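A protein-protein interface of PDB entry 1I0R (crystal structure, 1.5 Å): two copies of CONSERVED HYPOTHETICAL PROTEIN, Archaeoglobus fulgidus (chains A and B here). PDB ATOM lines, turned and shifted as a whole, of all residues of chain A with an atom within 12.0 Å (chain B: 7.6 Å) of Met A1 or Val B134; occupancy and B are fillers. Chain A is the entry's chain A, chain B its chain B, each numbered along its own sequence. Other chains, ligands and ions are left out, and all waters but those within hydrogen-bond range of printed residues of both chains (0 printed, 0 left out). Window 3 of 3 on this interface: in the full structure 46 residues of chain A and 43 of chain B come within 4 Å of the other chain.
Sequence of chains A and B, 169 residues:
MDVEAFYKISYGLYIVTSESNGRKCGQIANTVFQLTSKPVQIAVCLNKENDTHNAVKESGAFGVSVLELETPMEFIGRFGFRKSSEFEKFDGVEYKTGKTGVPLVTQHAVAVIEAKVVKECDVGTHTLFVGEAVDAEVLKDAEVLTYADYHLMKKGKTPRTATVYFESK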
ATOM      1  N   MET A   1     -22.855 -14.363  13.267  1.00  0.00           N
ATOM      2  CA  MET A   1     -21.615 -14.562  14.070  1.00  0.00           C
ATOM      3  C   MET A   1     -20.708 -13.335  13.980  1.00  0.00           C
ATOM      4  O   MET A   1     -20.240 -12.969  12.897  1.00  0.00           O
ATOM      5  CB  MET A   1     -20.887 -15.807  13.572  1.00  0.00           C
ATOM      6  CG  MET A   1     -19.714 -16.217  14.425  1.00  0.00           C
ATOM      7  SD  MET A   1     -19.283 -17.922  14.074  1.00  0.00           S
ATOM      8  CE  MET A   1     -18.268 -17.691  12.608  1.00  0.00           C
ATOM      9  N   ASP A   2     -20.465 -12.707  15.128  1.00  0.00           N
ATOM     10  CA  ASP A   2     -19.640 -11.508  15.215  1.00  0.00           C
ATOM     11  C   ASP A   2     -18.160 -11.838  15.431  1.00  0.00           C
ATOM     12  O   ASP A   2     -17.759 -12.283  16.504  1.00  0.00           O
ATOM     13  CB  ASP A   2     -20.153 -10.635  16.355  1.00  0.00           C
ATOM     14  CG  ASP A   2     -19.415  -9.315  16.468  1.00  0.00           C
ATOM     15  OD1 ASP A   2     -19.766  -8.537  17.378  1.00  0.00           O
ATOM     16  OD2 ASP A   2     -18.498  -9.051  15.655  1.00  0.00           O
ATOM     17  N   VAL A   3     -17.349 -11.614  14.407  1.00  0.00           N
ATOM     18  CA  VAL A   3     -15.923 -11.902  14.509  1.00  0.00           C
ATOM     19  C   VAL A   3     -15.225 -11.193  15.671  1.00  0.00           C
ATOM     20  O   VAL A   3     -14.229 -11.696  16.197  1.00  0.00           O
ATOM     21  CB  VAL A   3     -15.207 -11.552  13.190  1.00  0.00           C
ATOM     22  CG1 VAL A   3     -13.710 -11.709  13.354  1.00  0.00           C
ATOM     23  CG2 VAL A   3     -15.708 -12.467  12.088  1.00  0.00           C
ATOM     24  N   GLU A   4     -15.734 -10.033  16.069  1.00  0.00           N
ATOM     25  CA  GLU A   4     -15.156  -9.277  17.181  1.00  0.00           C
ATOM     26  C   GLU A   4     -15.161 -10.047  18.501  1.00  0.00           C
ATOM     27  O   GLU A   4     -14.380  -9.756  19.408  1.00  0.00           O
ATOM     28  CB  GLU A   4     -15.908  -7.954  17.370  1.00  0.00           C
ATOM     29  CG  GLU A   4     -15.534  -6.883  16.361  1.00  0.00           C
ATOM     30  CD  GLU A   4     -14.522  -5.885  16.899  1.00  0.00           C
ATOM     31  OE1 GLU A   4     -13.994  -5.094  16.085  1.00  0.00           O
ATOM     32  OE2 GLU A   4     -14.256  -5.880  18.129  1.00  0.00           O
ATOM     33  N   ALA A   5     -16.058 -11.018  18.626  1.00  0.00           N
ATOM     34  CA  ALA A   5     -16.121 -11.797  19.858  1.00  0.00           C
ATOM     35  C   ALA A   5     -14.817 -12.586  20.038  1.00  0.00           C
ATOM     36  O   ALA A   5     -14.341 -12.765  21.159  1.00  0.00           O
ATOM     37  CB  ALA A   5     -17.303 -12.753  19.812  1.00  0.00           C
ATOM     38  N   PHE A   6     -14.230 -13.034  18.936  1.00  0.00           N
ATOM     39  CA  PHE A   6     -12.990 -13.808  19.044  1.00  0.00           C
ATOM     40  C   PHE A   6     -11.822 -12.936  19.485  1.00  0.00           C
ATOM     41  O   PHE A   6     -10.831 -13.442  20.013  1.00  0.00           O
ATOM     42  CB  PHE A   6     -12.677 -14.517  17.714  1.00  0.00           C
ATOM     43  CG  PHE A   6     -13.839 -15.317  17.169  1.00  0.00           C
ATOM     44  CD1 PHE A   6     -14.472 -14.925  15.999  1.00  0.00           C
ATOM     45  CD2 PHE A   6     -14.332 -16.426  17.852  1.00  0.00           C
ATOM     46  CE1 PHE A   6     -15.590 -15.623  15.508  1.00  0.00           C
ATOM     47  CE2 PHE A   6     -15.448 -17.124  17.368  1.00  0.00           C
ATOM     48  CZ  PHE A   6     -16.071 -16.719  16.200  1.00  0.00           C
ATOM     49  N   TYR A   7     -11.952 -11.622  19.288  1.00  0.00           N
ATOM     50  CA  TYR A   7     -10.920 -10.663  19.689  1.00  0.00           C
ATOM     51  C   TYR A   7     -10.805 -10.592  21.208  1.00  0.00           C
ATOM     52  O   TYR A   7      -9.820 -10.083  21.741  1.00  0.00           O
ATOM     53  CB  TYR A   7     -11.255  -9.244  19.198  1.00  0.00           C
ATOM     54  CG  TYR A   7     -11.250  -9.015  17.698  1.00  0.00           C
ATOM     55  CD1 TYR A   7     -11.779  -7.832  17.170  1.00  0.00           C
ATOM     56  CD2 TYR A   7     -10.723  -9.955  16.812  1.00  0.00           C
ATOM     57  CE1 TYR A   7     -11.787  -7.589  15.791  1.00  0.00           C
ATOM     58  CE2 TYR A   7     -10.722  -9.719  15.421  1.00  0.00           C
ATOM     59  CZ  TYR A   7     -11.259  -8.530  14.927  1.00  0.00           C
ATOM     60  OH  TYR A   7     -11.265  -8.267  13.578  1.00  0.00           O
ATOM     61  N   LYS A   8     -11.825 -11.095  21.902  1.00  0.00           N
ATOM     62  CA  LYS A   8     -11.840 -11.073  23.354  1.00  0.00           C
ATOM     63  C   LYS A   8     -11.025 -12.186  24.024  1.00  0.00           C
ATOM     64  O   LYS A   8     -10.803 -12.144  25.243  1.00  0.00           O
ATOM     65  CB  LYS A   8     -13.280 -11.107  23.872  1.00  0.00           C
ATOM     66  CG  LYS A   8     -14.172  -9.959  23.343  1.00  0.00           C
ATOM     67  CD  LYS A   8     -13.606  -8.575  23.677  1.00  0.00           C
ATOM     68  CE  LYS A   8     -14.577  -7.467  23.218  1.00  0.00           C
ATOM     69  NZ  LYS A   8     -14.063  -6.109  23.595  1.00  0.00           N
ATOM     70  N   ILE A   9     -10.571 -13.163  23.238  1.00  0.00           N
ATOM     71  CA  ILE A   9      -9.743 -14.259  23.775  1.00  0.00           C
ATOM     72  C   ILE A   9      -8.332 -13.709  24.072  1.00  0.00           C
ATOM     73  O   ILE A   9      -7.770 -12.943  23.267  1.00  0.00           O
ATOM     74  CB  ILE A   9      -9.680 -15.427  22.753  1.00  0.00           C
ATOM     75  CG1 ILE A   9     -11.091 -16.008  22.592  1.00  0.00           C
ATOM     76  CG2 ILE A   9      -8.695 -16.508  23.212  1.00  0.00           C
ATOM     77  CD1 ILE A   9     -11.252 -16.964  21.432  1.00  0.00           C
ATOM     78  N   SER B  37      -8.674 -19.176  11.168  1.00  0.00           N
ATOM     79  CA  SER B  37      -9.686 -18.168  10.825  1.00  0.00           C
ATOM     80  C   SER B  37     -10.516 -18.596   9.619  1.00  0.00           C
ATOM     81  O   SER B  37     -11.587 -18.036   9.378  1.00  0.00           O
ATOM     82  CB  SER B  37      -9.028 -16.823  10.544  1.00  0.00           C
ATOM     83  OG  SER B  37      -8.119 -16.938   9.457  1.00  0.00           O
ATOM     84  N   PRO B  39     -12.025 -22.082   8.336  1.00  0.00           N
ATOM     85  CA  PRO B  39     -13.075 -21.332   9.026  1.00  0.00           C
ATOM     86  C   PRO B  39     -12.619 -21.067  10.461  1.00  0.00           C
ATOM     87  O   PRO B  39     -11.572 -21.555  10.890  1.00  0.00           O
ATOM     88  CB  PRO B  39     -14.254 -22.294   8.971  1.00  0.00           C
ATOM     89  CG  PRO B  39     -13.581 -23.616   9.177  1.00  0.00           C
ATOM     90  CD  PRO B  39     -12.336 -23.521   8.315  1.00  0.00           C
ATOM     91  N   VAL B  40     -13.394 -20.306  11.216  1.00  0.00           N
ATOM     92  CA  VAL B  40     -13.001 -20.049  12.582  1.00  0.00           C
ATOM     93  C   VAL B  40     -13.146 -21.317  13.431  1.00  0.00           C
ATOM     94  O   VAL B  40     -14.233 -21.917  13.508  1.00  0.00           O
ATOM     95  CB  VAL B  40     -13.844 -18.933  13.209  1.00  0.00           C
ATOM     96  CG1 VAL B  40     -13.527 -18.833  14.711  1.00  0.00           C
ATOM     97  CG2 VAL B  40     -13.519 -17.597  12.524  1.00  0.00           C
ATOM     98  N   GLN B  41     -12.028 -21.741  14.032  1.00  0.00           N
ATOM     99  CA  GLN B  41     -12.010 -22.894  14.926  1.00  0.00           C
ATOM    100  C   GLN B  41     -11.430 -22.475  16.272  1.00  0.00           C
ATOM    101  O   GLN B  41     -10.455 -21.710  16.349  1.00  0.00           O
ATOM    102  CB  GLN B  41     -11.187 -24.045  14.331  1.00  0.00           C
ATOM    103  CG  GLN B  41     -11.814 -24.566  13.073  1.00  0.00           C
ATOM    104  CD  GLN B  41     -11.004 -25.670  12.434  1.00  0.00           C
ATOM    105  OE1 GLN B  41      -9.867 -25.446  11.976  1.00  0.00           O
ATOM    106  NE2 GLN B  41     -11.573 -26.862  12.393  1.00  0.00           N
ATOM    107  N   ILE B  42     -12.045 -22.988  17.333  1.00  0.00           N
ATOM    108  CA  ILE B  42     -11.657 -22.686  18.721  1.00  0.00           C
ATOM    109  C   ILE B  42     -11.307 -23.976  19.437  1.00  0.00           C
ATOM    110  O   ILE B  42     -12.010 -24.975  19.300  1.00  0.00           O
ATOM    111  CB  ILE B  42     -12.830 -22.040  19.513  1.00  0.00           C
ATOM    112  CG1 ILE B  42     -13.362 -20.818  18.764  1.00  0.00           C
ATOM    113  CG2 ILE B  42     -12.373 -21.658  20.925  1.00  0.00           C
ATOM    114  CD1 ILE B  42     -12.307 -19.764  18.422  1.00  0.00           C
ATOM    115  N   ALA B  61     -20.461 -30.716  21.313  1.00  0.00           N
ATOM    116  CA  ALA B  61     -20.605 -29.265  21.246  1.00  0.00           C
ATOM    117  C   ALA B  61     -20.185 -28.602  22.544  1.00  0.00           C
ATOM    118  O   ALA B  61     -20.174 -29.237  23.590  1.00  0.00           O
ATOM    119  CB  ALA B  61     -22.062 -28.883  20.912  1.00  0.00           C
ATOM    120  N   PHE B  62     -19.803 -27.335  22.466  1.00  0.00           N
ATOM    121  CA  PHE B  62     -19.430 -26.602  23.663  1.00  0.00           C
ATOM    122  C   PHE B  62     -19.638 -25.108  23.519  1.00  0.00           C
ATOM    123  O   PHE B  62     -19.718 -24.570  22.395  1.00  0.00           O
ATOM    124  CB  PHE B  62     -17.955 -26.915  24.094  1.00  0.00           C
ATOM    125  CG  PHE B  62     -16.880 -26.438  23.127  1.00  0.00           C
ATOM    126  CD1 PHE B  62     -16.387 -25.131  23.188  1.00  0.00           C
ATOM    127  CD2 PHE B  62     -16.322 -27.322  22.205  1.00  0.00           C
ATOM    128  CE1 PHE B  62     -15.344 -24.718  22.325  1.00  0.00           C
ATOM    129  CE2 PHE B  62     -15.286 -26.930  21.347  1.00  0.00           C
ATOM    130  CZ  PHE B  62     -14.803 -25.630  21.410  1.00  0.00           C
ATOM    131  N   GLY B  98     -28.275 -22.287  22.902  1.00  0.00           N
ATOM    132  CA  GLY B  98     -28.018 -22.152  21.482  1.00  0.00           C
ATOM    133  C   GLY B  98     -28.580 -23.285  20.644  1.00  0.00           C
ATOM    134  O   GLY B  98     -29.055 -24.282  21.186  1.00  0.00           O
ATOM    135  N   LYS B  99     -28.506 -23.133  19.323  1.00  0.00           N
ATOM    136  CA  LYS B  99     -28.999 -24.157  18.403  1.00  0.00           C
ATOM    137  C   LYS B  99     -28.316 -25.516  18.627  1.00  0.00           C
ATOM    138  O   LYS B  99     -28.919 -26.565  18.402  1.00  0.00           O
ATOM    139  CB  LYS B  99     -28.807 -23.706  16.949  1.00  0.00           C
ATOM    140  CG  LYS B  99     -29.698 -22.548  16.535  1.00  0.00           C
ATOM    141  CD  LYS B  99     -29.528 -22.175  15.056  1.00  0.00           C
ATOM    142  CE  LYS B  99     -30.525 -21.082  14.677  1.00  0.00           C
ATOM    143  NZ  LYS B  99     -30.372 -20.581  13.273  1.00  0.00           N
ATOM    144  N   THR B 100     -27.066 -25.502  19.088  1.00  0.00           N
ATOM    145  CA  THR B 100     -26.350 -26.757  19.333  1.00  0.00           C
ATOM    146  C   THR B 100     -26.820 -27.463  20.593  1.00  0.00           C
ATOM    147  O   THR B 100     -26.451 -28.615  20.826  1.00  0.00           O
ATOM    148  CB  THR B 100     -24.844 -26.549  19.519  1.00  0.00           C
ATOM    149  OG1 THR B 100     -24.630 -25.886  20.772  1.00  0.00           O
ATOM    150  CG2 THR B 100     -24.254 -25.747  18.390  1.00  0.00           C
ATOM    151  N   VAL B 112     -19.695 -14.450  24.173  1.00  0.00           N
ATOM    152  CA  VAL B 112     -19.996 -15.876  24.198  1.00  0.00           C
ATOM    153  C   VAL B 112     -19.776 -16.443  22.811  1.00  0.00           C
ATOM    154  O   VAL B 112     -20.006 -15.762  21.801  1.00  0.00           O
ATOM    155  CB  VAL B 112     -21.450 -16.197  24.669  1.00  0.00           C
ATOM    156  CG1 VAL B 112     -21.572 -15.906  26.155  1.00  0.00           C
ATOM    157  CG2 VAL B 112     -22.478 -15.392  23.870  1.00  0.00           C
ATOM    158  N   ILE B 113     -19.298 -17.684  22.763  1.00  0.00           N
ATOM    159  CA  ILE B 113     -19.030 -18.370  21.514  1.00  0.00           C
ATOM    160  C   ILE B 113     -19.633 -19.752  21.608  1.00  0.00           C
ATOM    161  O   ILE B 113     -19.574 -20.380  22.666  1.00  0.00           O
ATOM    162  CB  ILE B 113     -17.491 -18.504  21.310  1.00  0.00           C
ATOM    163  CG1 ILE B 113     -16.868 -17.108  21.280  1.00  0.00           C
ATOM    164  CG2 ILE B 113     -17.180 -19.321  20.076  1.00  0.00           C
ATOM    165  CD1 ILE B 113     -15.337 -17.133  21.389  1.00  0.00           C
ATOM    166  N   GLU B 114     -20.229 -20.213  20.510  1.00  0.00           N
ATOM    167  CA  GLU B 114     -20.825 -21.538  20.454  1.00  0.00           C
ATOM    168  C   GLU B 114     -20.063 -22.300  19.375  1.00  0.00           C
ATOM    169  O   GLU B 114     -19.773 -21.740  18.303  1.00  0.00           O
ATOM    170  CB  GLU B 114     -22.316 -21.405  20.107  1.00  0.00           C
ATOM    171  CG  GLU B 114     -23.067 -22.696  19.999  1.00  0.00           C
ATOM    172  CD  GLU B 114     -24.561 -22.467  19.765  1.00  0.00           C
ATOM    173  OE1 GLU B 114     -24.938 -21.371  19.292  1.00  0.00           O
ATOM    174  OE2 GLU B 114     -25.340 -23.394  20.050  1.00  0.00           O
ATOM    175  N   ALA B 115     -19.718 -23.562  19.646  1.00  0.00           N
ATOM    176  CA  ALA B 115     -18.953 -24.354  18.672  1.00  0.00           C
ATOM    177  C   ALA B 115     -19.360 -25.824  18.573  1.00  0.00           C
ATOM    178  O   ALA B 115     -19.838 -26.401  19.548  1.00  0.00           O
ATOM    179  CB  ALA B 115     -17.427 -24.261  19.014  1.00  0.00           C
ATOM    180  N   LYS B 116     -19.212 -26.419  17.386  1.00  0.00           N
ATOM    181  CA  LYS B 116     -19.489 -27.847  17.224  1.00  0.00           C
ATOM    182  C   LYS B 116     -18.110 -28.515  17.079  1.00  0.00           C
ATOM    183  O   LYS B 116     -17.259 -28.015  16.334  1.00  0.00           O
ATOM    184  CB  LYS B 116     -20.358 -28.161  15.986  1.00  0.00           C
ATOM    185  CG  LYS B 116     -19.715 -27.826  14.651  1.00  0.00           C
ATOM    186  CD  LYS B 116     -20.512 -28.378  13.467  1.00  0.00           C
ATOM    187  CE  LYS B 116     -19.674 -28.299  12.169  1.00  0.00           C
ATOM    188  NZ  LYS B 116     -20.419 -28.776  10.949  1.00  0.00           N
ATOM    189  N   VAL B 117     -17.895 -29.599  17.813  1.00  0.00           N
ATOM    190  CA  VAL B 117     -16.621 -30.324  17.769  1.00  0.00           C
ATOM    191  C   VAL B 117     -16.379 -30.988  16.426  1.00  0.00           C
ATOM    192  O   VAL B 117     -17.212 -31.773  15.943  1.00  0.00           O
ATOM    193  CB  VAL B 117     -16.536 -31.418  18.873  1.00  0.00           C
ATOM    194  CG1 VAL B 117     -15.191 -32.213  18.730  1.00  0.00           C
ATOM    195  CG2 VAL B 117     -16.652 -30.770  20.258  1.00  0.00           C
ATOM    196  N   GLY B 131     -13.251 -27.046  18.010  1.00  0.00           N
ATOM    197  CA  GLY B 131     -14.605 -26.777  17.564  1.00  0.00           C
ATOM    198  C   GLY B 131     -14.714 -25.732  16.476  1.00  0.00           C
ATOM    199  O   GLY B 131     -13.975 -24.744  16.451  1.00  0.00           O
ATOM    200  N   GLU B 132     -15.659 -25.927  15.567  1.00  0.00           N
ATOM    201  CA  GLU B 132     -15.874 -24.939  14.530  1.00  0.00           C
ATOM    202  C   GLU B 132     -16.902 -23.971  15.122  1.00  0.00           C
ATOM    203  O   GLU B 132     -17.949 -24.410  15.586  1.00  0.00           O
ATOM    204  CB  GLU B 132     -16.417 -25.607  13.268  1.00  0.00           C
ATOM    205  CG  GLU B 132     -16.454 -24.663  12.092  1.00  0.00           C
ATOM    206  CD  GLU B 132     -16.834 -25.346  10.777  1.00  0.00           C
ATOM    207  OE1 GLU B 132     -16.258 -26.416  10.443  1.00  0.00           O
ATOM    208  OE2 GLU B 132     -17.705 -24.793  10.073  1.00  0.00           O
ATOM    209  N   ALA B 133     -16.604 -22.679  15.134  1.00  0.00           N
ATOM    210  CA  ALA B 133     -17.529 -21.689  15.698  1.00  0.00           C
ATOM    211  C   ALA B 133     -18.794 -21.590  14.850  1.00  0.00           C
ATOM    212  O   ALA B 133     -18.723 -21.443  13.629  1.00  0.00           O
ATOM    213  CB  ALA B 133     -16.841 -20.319  15.797  1.00  0.00           C
ATOM    214  N   VAL B 134     -19.952 -21.684  15.500  1.00  0.00           N
ATOM    215  CA  VAL B 134     -21.222 -21.581  14.765  1.00  0.00           C
ATOM    216  C   VAL B 134     -21.997 -20.307  15.110  1.00  0.00           C
ATOM    217  O   VAL B 134     -22.924 -19.938  14.392  1.00  0.00           O
ATOM    218  CB  VAL B 134     -22.098 -22.830  14.970  1.00  0.00           C
ATOM    219  CG1 VAL B 134     -21.422 -24.029  14.302  1.00  0.00           C
ATOM    220  CG2 VAL B 134     -22.323 -23.105  16.453  1.00  0.00           C
ATOM    221  N   ASP B 135     -21.644 -19.664  16.219  1.00  0.00           N
ATOM    222  CA  ASP B 135     -22.221 -18.372  16.602  1.00  0.00           C
ATOM    223  C   ASP B 135     -21.266 -17.718  17.578  1.00  0.00           C
ATOM    224  O   ASP B 135     -20.441 -18.398  18.205  1.00  0.00           O
ATOM    225  CB  ASP B 135     -23.604 -18.500  17.264  1.00  0.00           C
ATOM    226  CG  ASP B 135     -24.383 -17.172  17.246  1.00  0.00           C
ATOM    227  OD1 ASP B 135     -25.433 -17.083  17.932  1.00  0.00           O
ATOM    228  OD2 ASP B 135     -23.958 -16.213  16.548  1.00  0.00           O
ATOM    229  N   ALA B 136     -21.355 -16.401  17.697  1.00  0.00           N
ATOM    230  CA  ALA B 136     -20.503 -15.676  18.608  1.00  0.00           C
ATOM    231  C   ALA B 136     -21.053 -14.271  18.705  1.00  0.00           C
ATOM    232  O   ALA B 136     -21.505 -13.704  17.698  1.00  0.00           O
ATOM    233  CB  ALA B 136     -19.067 -15.650  18.078  1.00  0.00           C
ATOM    234  N   GLU B 137     -21.032 -13.710  19.906  1.00  0.00           N
ATOM    235  CA  GLU B 137     -21.526 -12.358  20.099  1.00  0.00           C
ATOM    236  C   GLU B 137     -20.819 -11.612  21.221  1.00  0.00           C
ATOM    237  O   GLU B 137     -20.379 -12.215  22.212  1.00  0.00           O
ATOM    238  CB  GLU B 137     -23.034 -12.392  20.361  1.00  0.00           C
ATOM    239  CG  GLU B 137     -23.464 -13.152  21.608  1.00  0.00           C
ATOM    240  CD  GLU B 137     -24.983 -13.317  21.675  1.00  0.00           C
ATOM    241  OE1 GLU B 137     -25.488 -14.436  21.407  1.00  0.00           O
ATOM    242  OE2 GLU B 137     -25.664 -12.312  21.973  1.00  0.00           O
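Val B134 touches Met A1. Met A1 touches Ala B136. Ala A5 touches Ala B136. Glu B137 touches Ala A5 (N to CB, 3.9 Å). Phe A6 touches Val B40. CD2 of Phe A6 touches CD1 of Ile B42, at 3.9 Å. CD2 of Phe A6 touches CD1 of Ile B113, at 3.7 Å. Ala B133 touches Phe A6 (CB to CZ, 3.7 Å). CZ of Phe A6 touches CB of Ala B136, 3.7 Å away.
Met A1 touches just these residues of chain B: Ala B133 (3.6 Å), Val B134 (3.8 Å), Asp B135 (3.6 Å) and Ala B136 (3.7 Å). Of the printed residues of chain B, Asp A2 touches Ala B136. Printed residues of chain B within 4 Å of Phe A6: Val B40 (3.6 Å), Ile B42 (3.9 Å), Ile B113 (3.7 Å), Ala B133 (3.7 Å) and Ala B136 (3.7 Å). Val B40 touches one residue of chain A. No residue of chain A comes within 4 Å of Lys B99. No residue of chain A comes within 4 Å of Glu B114. No residue of chain A comes within 4 Å of Ala B115. No residue of chain A comes within 4 Å of Lys B116. Glu B132 touches none of the printed residues of chain A. Ala B133 touches two residues of chain A. Val B134 touches just one residue of chain A: Met A1 (3.8 Å). Printed residues of chain A within 4 Å of Asp B135: Met A1. Ala B136 touches just these residues of chain A: Met A1 (3.7 Å), Asp A2 (2.9 Å), Ala A5 (3.8 Å) and Phe A6 (3.7 Å). The nearest residue of chain B that does not touch Met A1 is Val B40 (4.6 Å). The nearest residue of chain A that does not touch Val B134 is Phe A6 (6.3 Å).
Printed residues of chain B that touch a printed residue of chain A: Val B40, Ile B42, Ile B113, Ala B133, Val B134, Asp B135, Ala B136 and Glu B137. Hydrophobic or aromatic side chains of chain B within 4 Å of the printed part of chain A: Val B40, Ile B42, Ile B113, Ala B133 and Ala B136. Of the 9 printed residues of chain A, 4 touch a printed residue of chain B. Printed residues of chain A that touch a printed residue of chain B: Met A1, Asp A2, Ala A5 and Phe A6.
No position is printed for both chains. Of the 12 pairs that touch across the chains among the printed residues, none has its exchanged pair printed and touching as well.
SD of Met A1 sits at hydrogen-bond distance from N of Asp B135. N of Asp A2 lies within hydrogen-bond range of O of Ala B136 (2.9 Å). The side-chain sulfur (SD) of Met A1 lies close to the backbone carbonyl oxygen (O) of Ala B133 (3.6 Å).
The backbone NH (N) of Glu A4 sits at hydrogen-bond distance from the side-chain carboxylate (OD2) of Asp A2 (3.0 Å). The backbone NH of Ala B133 sits at hydrogen-bond distance from the backbone carbonyl oxygen of Val B40, 3.0 Å away. The backbone NH (N) of Gly B131 lies within hydrogen-bond range of the backbone carbonyl oxygen (O) of Ile B42. N of Glu B137 is in hydrogen-bond range of O of Val B112. O of Glu B114 lies within hydrogen-bond range of N of Val B134 (2.8 Å). N of Glu B114 sits at hydrogen-bond distance from O of Asp B135 (2.9 Å).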
